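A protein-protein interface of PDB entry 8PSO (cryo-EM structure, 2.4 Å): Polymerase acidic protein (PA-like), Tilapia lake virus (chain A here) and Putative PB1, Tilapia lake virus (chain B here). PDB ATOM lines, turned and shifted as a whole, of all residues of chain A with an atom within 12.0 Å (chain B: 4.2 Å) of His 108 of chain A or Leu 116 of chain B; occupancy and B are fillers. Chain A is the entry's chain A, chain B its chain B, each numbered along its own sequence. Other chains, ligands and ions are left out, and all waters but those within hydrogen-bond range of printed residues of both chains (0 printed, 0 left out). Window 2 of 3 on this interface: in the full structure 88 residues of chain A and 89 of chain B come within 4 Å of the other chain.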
ATOM      1  N   GLY A 102      32.806  16.212   4.752  1.00  0.00           N
ATOM      2  CA  GLY A 102      31.358  16.322   4.736  1.00  0.00           C
ATOM      3  C   GLY A 102      30.756  16.329   6.126  1.00  0.00           C
ATOM      4  O   GLY A 102      29.718  16.947   6.360  1.00  0.00           O
ATOM      5  N   VAL A 103      31.411  15.634   7.056  1.00  0.00           N
ATOM      6  CA  VAL A 103      30.931  15.579   8.431  1.00  0.00           C
ATOM      7  C   VAL A 103      31.130  16.939   9.086  1.00  0.00           C
ATOM      8  O   VAL A 103      32.198  17.553   8.971  1.00  0.00           O
ATOM      9  CB  VAL A 103      31.650  14.467   9.208  1.00  0.00           C
ATOM     10  CG1 VAL A 103      33.085  14.870   9.519  1.00  0.00           C
ATOM     11  CG2 VAL A 103      30.892  14.137  10.486  1.00  0.00           C
ATOM     12  N   VAL A 104      30.094  17.420   9.776  1.00  0.00           N
ATOM     13  CA  VAL A 104      30.159  18.737  10.395  1.00  0.00           C
ATOM     14  C   VAL A 104      31.227  18.736  11.478  1.00  0.00           C
ATOM     15  O   VAL A 104      31.296  17.821  12.308  1.00  0.00           O
ATOM     16  CB  VAL A 104      28.787  19.131  10.960  1.00  0.00           C
ATOM     17  CG1 VAL A 104      28.863  20.488  11.647  1.00  0.00           C
ATOM     18  CG2 VAL A 104      27.742  19.148   9.854  1.00  0.00           C
ATOM     19  N   LYS A 105      32.067  19.765  11.471  1.00  0.00           N
ATOM     20  CA  LYS A 105      33.129  19.924  12.452  1.00  0.00           C
ATOM     21  C   LYS A 105      32.705  20.933  13.514  1.00  0.00           C
ATOM     22  O   LYS A 105      31.852  21.791  13.275  1.00  0.00           O
ATOM     23  CB  LYS A 105      34.428  20.382  11.784  1.00  0.00           C
ATOM     24  CG  LYS A 105      34.806  19.594  10.536  1.00  0.00           C
ATOM     25  CD  LYS A 105      36.028  18.724  10.777  1.00  0.00           C
ATOM     26  CE  LYS A 105      36.278  17.779   9.613  1.00  0.00           C
ATOM     27  NZ  LYS A 105      36.157  16.349  10.011  1.00  0.00           N
ATOM     28  N   VAL A 106      33.316  20.822  14.695  1.00  0.00           N
ATOM     29  CA  VAL A 106      32.947  21.699  15.802  1.00  0.00           C
ATOM     30  C   VAL A 106      33.229  23.153  15.456  1.00  0.00           C
ATOM     31  O   VAL A 106      32.498  24.054  15.882  1.00  0.00           O
ATOM     32  CB  VAL A 106      33.679  21.271  17.090  1.00  0.00           C
ATOM     33  CG1 VAL A 106      35.163  21.598  17.002  1.00  0.00           C
ATOM     34  CG2 VAL A 106      33.048  21.939  18.303  1.00  0.00           C
ATOM     35  N   GLY A 107      34.280  23.409  14.684  1.00  0.00           N
ATOM     36  CA  GLY A 107      34.622  24.742  14.243  1.00  0.00           C
ATOM     37  C   GLY A 107      33.862  25.214  13.023  1.00  0.00           C
ATOM     38  O   GLY A 107      34.227  26.239  12.441  1.00  0.00           O
ATOM     39  N   HIS A 108      32.817  24.495  12.619  1.00  0.00           N
ATOM     40  CA  HIS A 108      32.063  24.857  11.428  1.00  0.00           C
ATOM     41  C   HIS A 108      31.526  26.279  11.542  1.00  0.00           C
ATOM     42  O   HIS A 108      30.993  26.675  12.581  1.00  0.00           O
ATOM     43  CB  HIS A 108      30.912  23.872  11.225  1.00  0.00           C
ATOM     44  CG  HIS A 108      30.038  24.194  10.053  1.00  0.00           C
ATOM     45  ND1 HIS A 108      28.979  25.073  10.134  1.00  0.00           N
ATOM     46  CD2 HIS A 108      30.064  23.754   8.774  1.00  0.00           C
ATOM     47  CE1 HIS A 108      28.392  25.161   8.954  1.00  0.00           C
ATOM     48  NE2 HIS A 108      29.031  24.370   8.111  1.00  0.00           N
ATOM     49  N   LYS A 109      31.673  27.045  10.464  1.00  0.00           N
ATOM     50  CA  LYS A 109      31.216  28.427  10.404  1.00  0.00           C
ATOM     51  C   LYS A 109      29.898  28.482   9.642  1.00  0.00           C
ATOM     52  O   LYS A 109      29.839  28.097   8.469  1.00  0.00           O
ATOM     53  CB  LYS A 109      32.264  29.314   9.732  1.00  0.00           C
ATOM     54  CG  LYS A 109      32.250  30.758  10.201  1.00  0.00           C
ATOM     55  CD  LYS A 109      33.376  31.558   9.565  1.00  0.00           C
ATOM     56  CE  LYS A 109      33.088  31.875   8.106  1.00  0.00           C
ATOM     57  NZ  LYS A 109      32.866  33.331   7.883  1.00  0.00           N
ATOM     58  N   ALA A 110      28.852  28.961  10.304  1.00  0.00           N
ATOM     59  CA  ALA A 110      27.530  29.040   9.707  1.00  0.00           C
ATOM     60  C   ALA A 110      27.378  30.327   8.896  1.00  0.00           C
ATOM     61  O   ALA A 110      28.240  31.208   8.906  1.00  0.00           O
ATOM     62  CB  ALA A 110      26.453  28.959  10.787  1.00  0.00           C
ATOM     63  N   SER A 111      26.254  30.424   8.184  1.00  0.00           N
ATOM     64  CA  SER A 111      25.997  31.601   7.360  1.00  0.00           C
ATOM     65  C   SER A 111      25.618  32.810   8.205  1.00  0.00           C
ATOM     66  O   SER A 111      25.833  33.951   7.782  1.00  0.00           O
ATOM     67  CB  SER A 111      24.893  31.298   6.348  1.00  0.00           C
ATOM     68  OG  SER A 111      24.147  30.159   6.735  1.00  0.00           O
ATOM     69  N   TYR A 112      25.055  32.585   9.389  1.00  0.00           N
ATOM     70  CA  TYR A 112      24.648  33.659  10.285  1.00  0.00           C
ATOM     71  C   TYR A 112      25.749  34.053  11.263  1.00  0.00           C
ATOM     72  O   TYR A 112      25.508  34.882  12.147  1.00  0.00           O
ATOM     73  CB  TYR A 112      23.390  33.253  11.059  1.00  0.00           C
ATOM     74  CG  TYR A 112      23.468  31.880  11.692  1.00  0.00           C
ATOM     75  CD1 TYR A 112      24.181  31.674  12.864  1.00  0.00           C
ATOM     76  CD2 TYR A 112      22.832  30.790  11.113  1.00  0.00           C
ATOM     77  CE1 TYR A 112      24.256  30.424  13.444  1.00  0.00           C
ATOM     78  CE2 TYR A 112      22.903  29.536  11.686  1.00  0.00           C
ATOM     79  CZ  TYR A 112      23.616  29.359  12.851  1.00  0.00           C
ATOM     80  OH  TYR A 112      23.689  28.111  13.426  1.00  0.00           O
ATOM     81  N   ASP A 113      26.945  33.477  11.125  1.00  0.00           N
ATOM     82  CA  ASP A 113      28.027  33.766  12.063  1.00  0.00           C
ATOM     83  C   ASP A 113      28.342  35.257  12.101  1.00  0.00           C
ATOM     84  O   ASP A 113      28.436  35.857  13.179  1.00  0.00           O
ATOM     85  CB  ASP A 113      29.269  32.963  11.675  1.00  0.00           C
ATOM     86  CG  ASP A 113      30.317  32.945  12.767  1.00  0.00           C
ATOM     87  OD1 ASP A 113      30.763  34.033  13.186  1.00  0.00           O
ATOM     88  OD2 ASP A 113      30.698  31.839  13.206  1.00  0.00           O
ATOM     89  N   ALA A 114      28.511  35.874  10.929  1.00  0.00           N
ATOM     90  CA  ALA A 114      28.858  37.291  10.885  1.00  0.00           C
ATOM     91  C   ALA A 114      27.741  38.149  11.463  1.00  0.00           C
ATOM     92  O   ALA A 114      28.005  39.138  12.156  1.00  0.00           O
ATOM     93  CB  ALA A 114      29.169  37.710   9.449  1.00  0.00           C
ATOM     94  N   LEU A 116      25.575  37.321  13.819  1.00  0.00           N
ATOM     95  CA  LEU A 116      25.595  37.199  15.272  1.00  0.00           C
ATOM     96  C   LEU A 116      26.787  37.934  15.871  1.00  0.00           C
ATOM     97  O   LEU A 116      26.677  38.530  16.947  1.00  0.00           O
ATOM     98  CB  LEU A 116      25.612  35.725  15.675  1.00  0.00           C
ATOM     99  CG  LEU A 116      24.297  34.960  15.499  1.00  0.00           C
ATOM    100  CD1 LEU A 116      24.467  33.515  15.936  1.00  0.00           C
ATOM    101  CD2 LEU A 116      23.162  35.622  16.266  1.00  0.00           C
ATOM    102  N   ARG A 117      27.936  37.899  15.196  1.00  0.00           N
ATOM    103  CA  ARG A 117      29.094  38.636  15.691  1.00  0.00           C
ATOM    104  C   ARG A 117      28.834  40.138  15.679  1.00  0.00           C
ATOM    105  O   ARG A 117      29.207  40.848  16.619  1.00  0.00           O
ATOM    106  CB  ARG A 117      30.331  38.289  14.864  1.00  0.00           C
ATOM    107  CG  ARG A 117      30.974  36.973  15.271  1.00  0.00           C
ATOM    108  CD  ARG A 117      32.262  36.711  14.516  1.00  0.00           C
ATOM    109  NE  ARG A 117      32.762  35.361  14.751  1.00  0.00           N
ATOM    110  CZ  ARG A 117      33.448  34.989  15.824  1.00  0.00           C
ATOM    111  NH1 ARG A 117      33.740  35.843  16.790  1.00  0.00           N
ATOM    112  NH2 ARG A 117      33.850  33.726  15.931  1.00  0.00           N
ATOM    113  N   LEU B  62      32.052  17.053  15.068  1.00  0.00           N
ATOM    114  CA  LEU B  62      31.022  17.423  16.033  1.00  0.00           C
ATOM    115  C   LEU B  62      30.399  16.158  16.610  1.00  0.00           C
ATOM    116  O   LEU B  62      29.688  15.431  15.910  1.00  0.00           O
ATOM    117  CB  LEU B  62      29.966  18.299  15.365  1.00  0.00           C
ATOM    118  CG  LEU B  62      28.949  18.991  16.278  1.00  0.00           C
ATOM    119  CD1 LEU B  62      29.625  19.686  17.452  1.00  0.00           C
ATOM    120  CD2 LEU B  62      28.117  19.979  15.479  1.00  0.00           C
ATOM    121  N   ILE B 112      21.649  19.639  16.181  1.00  0.00           N
ATOM    122  CA  ILE B 112      22.777  20.563  16.124  1.00  0.00           C
ATOM    123  C   ILE B 112      23.300  20.672  14.697  1.00  0.00           C
ATOM    124  O   ILE B 112      23.664  21.763  14.239  1.00  0.00           O
ATOM    125  CB  ILE B 112      23.880  20.145  17.116  1.00  0.00           C
ATOM    126  CG1 ILE B 112      24.815  21.325  17.393  1.00  0.00           C
ATOM    127  CG2 ILE B 112      24.687  18.961  16.600  1.00  0.00           C
ATOM    128  CD1 ILE B 112      25.671  21.148  18.626  1.00  0.00           C
ATOM    129  N   CYS B 113      23.339  19.555  13.964  1.00  0.00           N
ATOM    130  CA  CYS B 113      23.746  19.624  12.563  1.00  0.00           C
ATOM    131  C   CYS B 113      22.789  20.493  11.756  1.00  0.00           C
ATOM    132  O   CYS B 113      23.222  21.339  10.963  1.00  0.00           O
ATOM    133  CB  CYS B 113      23.824  18.217  11.971  1.00  0.00           C
ATOM    134  SG  CYS B 113      25.327  17.314  12.411  1.00  0.00           S
ATOM    135  N   LYS B 114      21.481  20.311  11.957  1.00  0.00           N
ATOM    136  CA  LYS B 114      20.507  21.137  11.252  1.00  0.00           C
ATOM    137  C   LYS B 114      20.697  22.610  11.586  1.00  0.00           C
ATOM    138  O   LYS B 114      20.676  23.465  10.694  1.00  0.00           O
ATOM    139  CB  LYS B 114      19.089  20.691  11.609  1.00  0.00           C
ATOM    140  CG  LYS B 114      18.563  19.542  10.772  1.00  0.00           C
ATOM    141  CD  LYS B 114      17.128  19.215  11.145  1.00  0.00           C
ATOM    142  CE  LYS B 114      16.708  17.849  10.633  1.00  0.00           C
ATOM    143  NZ  LYS B 114      15.326  17.500  11.063  1.00  0.00           N
ATOM    144  N   VAL B 115      20.895  22.923  12.868  1.00  0.00           N
ATOM    145  CA  VAL B 115      21.087  24.310  13.278  1.00  0.00           C
ATOM    146  C   VAL B 115      22.327  24.892  12.613  1.00  0.00           C
ATOM    147  O   VAL B 115      22.331  26.050  12.176  1.00  0.00           O
ATOM    148  CB  VAL B 115      21.173  24.404  14.813  1.00  0.00           C
ATOM    149  CG1 VAL B 115      21.750  25.746  15.240  1.00  0.00           C
ATOM    150  CG2 VAL B 115      19.803  24.183  15.437  1.00  0.00           C
ATOM    151  N   LEU B 116      23.402  24.106  12.532  1.00  0.00           N
ATOM    152  CA  LEU B 116      24.642  24.609  11.957  1.00  0.00           C
ATOM    153  C   LEU B 116      24.587  24.706  10.437  1.00  0.00           C
ATOM    154  O   LEU B 116      25.396  25.433   9.852  1.00  0.00           O
ATOM    155  CB  LEU B 116      25.812  23.716  12.372  1.00  0.00           C
ATOM    156  CG  LEU B 116      26.368  23.931  13.781  1.00  0.00           C
ATOM    157  CD1 LEU B 116      27.487  22.944  14.062  1.00  0.00           C
ATOM    158  CD2 LEU B 116      26.859  25.359  13.974  1.00  0.00           C
ATOM    159  N   THR B 117      23.662  24.003   9.786  1.00  0.00           N
ATOM    160  CA  THR B 117      23.586  23.975   8.329  1.00  0.00           C
ATOM    161  C   THR B 117      22.287  24.587   7.811  1.00  0.00           C
ATOM    162  O   THR B 117      21.622  24.022   6.940  1.00  0.00           O
ATOM    163  CB  THR B 117      23.742  22.549   7.804  1.00  0.00           C
ATOM    164  OG1 THR B 117      22.590  21.773   8.161  1.00  0.00           O
ATOM    165  CG2 THR B 117      24.998  21.898   8.371  1.00  0.00           C
ATOM    166  N   VAL B 118      21.905  25.751   8.338  1.00  0.00           N
ATOM    167  CA  VAL B 118      20.788  26.520   7.796  1.00  0.00           C
ATOM    168  C   VAL B 118      21.349  27.700   7.017  1.00  0.00           C
ATOM    169  O   VAL B 118      22.458  28.178   7.279  1.00  0.00           O
ATOM    170  CB  VAL B 118      19.815  27.003   8.895  1.00  0.00           C
ATOM    171  CG1 VAL B 118      19.041  25.834   9.479  1.00  0.00           C
ATOM    172  CG2 VAL B 118      20.559  27.762   9.983  1.00  0.00           C
ATOM    173  N   SER B 237      30.791  28.761  15.324  1.00  0.00           N
ATOM    174  CA  SER B 237      29.429  29.266  15.448  1.00  0.00           C
ATOM    175  C   SER B 237      28.762  28.804  16.736  1.00  0.00           C
ATOM    176  O   SER B 237      27.915  29.520  17.277  1.00  0.00           O
ATOM    177  CB  SER B 237      28.599  28.835  14.240  1.00  0.00           C
ATOM    178  OG  SER B 237      28.841  29.681  13.131  1.00  0.00           O
ATOM    179  N   ILE B 238      29.116  27.623  17.243  1.00  0.00           N
ATOM    180  CA  ILE B 238      28.552  27.172  18.513  1.00  0.00           C
ATOM    181  C   ILE B 238      28.957  28.126  19.631  1.00  0.00           C
ATOM    182  O   ILE B 238      28.125  28.565  20.436  1.00  0.00           O
ATOM    183  CB  ILE B 238      28.992  25.728  18.811  1.00  0.00           C
ATOM    184  CG1 ILE B 238      28.097  24.740  18.063  1.00  0.00           C
ATOM    185  CG2 ILE B 238      28.946  25.444  20.307  1.00  0.00           C
ATOM    186  CD1 ILE B 238      28.718  23.376  17.876  1.00  0.00           C
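The backbone carbonyl oxygen of Val 104 of chain A sits at hydrogen-bond distance from the backbone NH of Leu 62 of chain B (3.0 Å).
O of His 108 of chain A lies within hydrogen-bond range of N of Ser 237 of chain B (3.5 Å).
The backbone NH of Ala 110 of chain A is in hydrogen-bond range of the side-chain hydroxyl of Ser 237 of chain B, 2.9 Å away.
OG of Ser 111 of chain A is in hydrogen-bond range of O of Val 118 of chain B (2.7 Å).
OH of Tyr 112 of chain A is in hydrogen-bond range of O of Val 115 of chain B (2.8 Å).
The side-chain hydroxyl of Ser 237 of chain B lies within hydrogen-bond range of the side-chain carboxylate of Asp 113 of chain A, at 2.8 Å.
The side-chain carboxylate (OD1) of Asp 113 of chain A is in salt-bridge range of the guanidinium group (NE) of Arg 117 of chain A, at 2.9 Å.
O of Cys 113 of chain B sits at hydrogen-bond distance from OG1 of Thr 117 of chain B (2.9 Å).
SG of Cys 113 of chain B touches CG2 of Val 104 of chain A, at 3.97 Å.
CD1 of Leu 116 of chain B touches CG1 of Val 104 of chain A, 3.7 Å away.
N of Val 106 of chain A touches N of Leu 62 of chain B, at 3.99 Å.
CE1 of His 108 of chain A touches O of Leu 116 of chain B (3.1 Å).
Ser 237 of chain B touches Lys 109 of chain A.
Leu 116 of chain B touches Ala 110 of chain A (O to CB, 3.8 Å).
Tyr 112 of chain A touches Leu 116 of chain B.
Val 118 of chain B touches Tyr 112 of chain A.
Of chain B, only Leu 116 and Ser 237 come within 4 Å of His 108 of chain A.
Of chain A, only Val 104 (3.7 Å), His 108 (3.1 Å), Ala 110 (3.8 Å) and Tyr 112 (3.9 Å) come within 4 Å of Leu 116 of chain B.
No residue of chain A comes within 4 Å of Ile 112 of chain B.
Cys 113 of chain B touches one residue of chain A.
No residue of chain A comes within 4 Å of Thr 117 of chain B.
Of chain A, only Ser 111 and Tyr 112 come within 4 Å of Val 118 of chain B.
No residue of chain A comes within 4 Å of Ile 238 of chain B.
Of the printed residues of chain A, Leu 62 of chain B touches Val 104 and Val 106.
Printed residues of chain B within 4 Å of Asp 113 of chain A: Ser 237 (2.8 Å).
Printed residues of chain B within 4 Å of Val 106 of chain A: Leu 62.
Lys 105 of chain A touches none of the printed residues of chain B.
Lys 114 of chain B touches none of the printed residues of chain A.
The nearest printed residue of chain B that does not touch His 108 of chain A is Thr 117 of chain B (4.7 Å).
The nearest printed residue of chain B that does not touch Ala 110 of chain A is Val 115 of chain B (5.2 Å).
Hydrophobic or aromatic side chains of chain A that line the printed part of chain B: Val 104, His 108, Ala 110 and Tyr 112.
Among the printed residues, no Asp or Glu carboxylate lies within 4 Å of a Lys or Arg side-chain nitrogen of the other chain.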
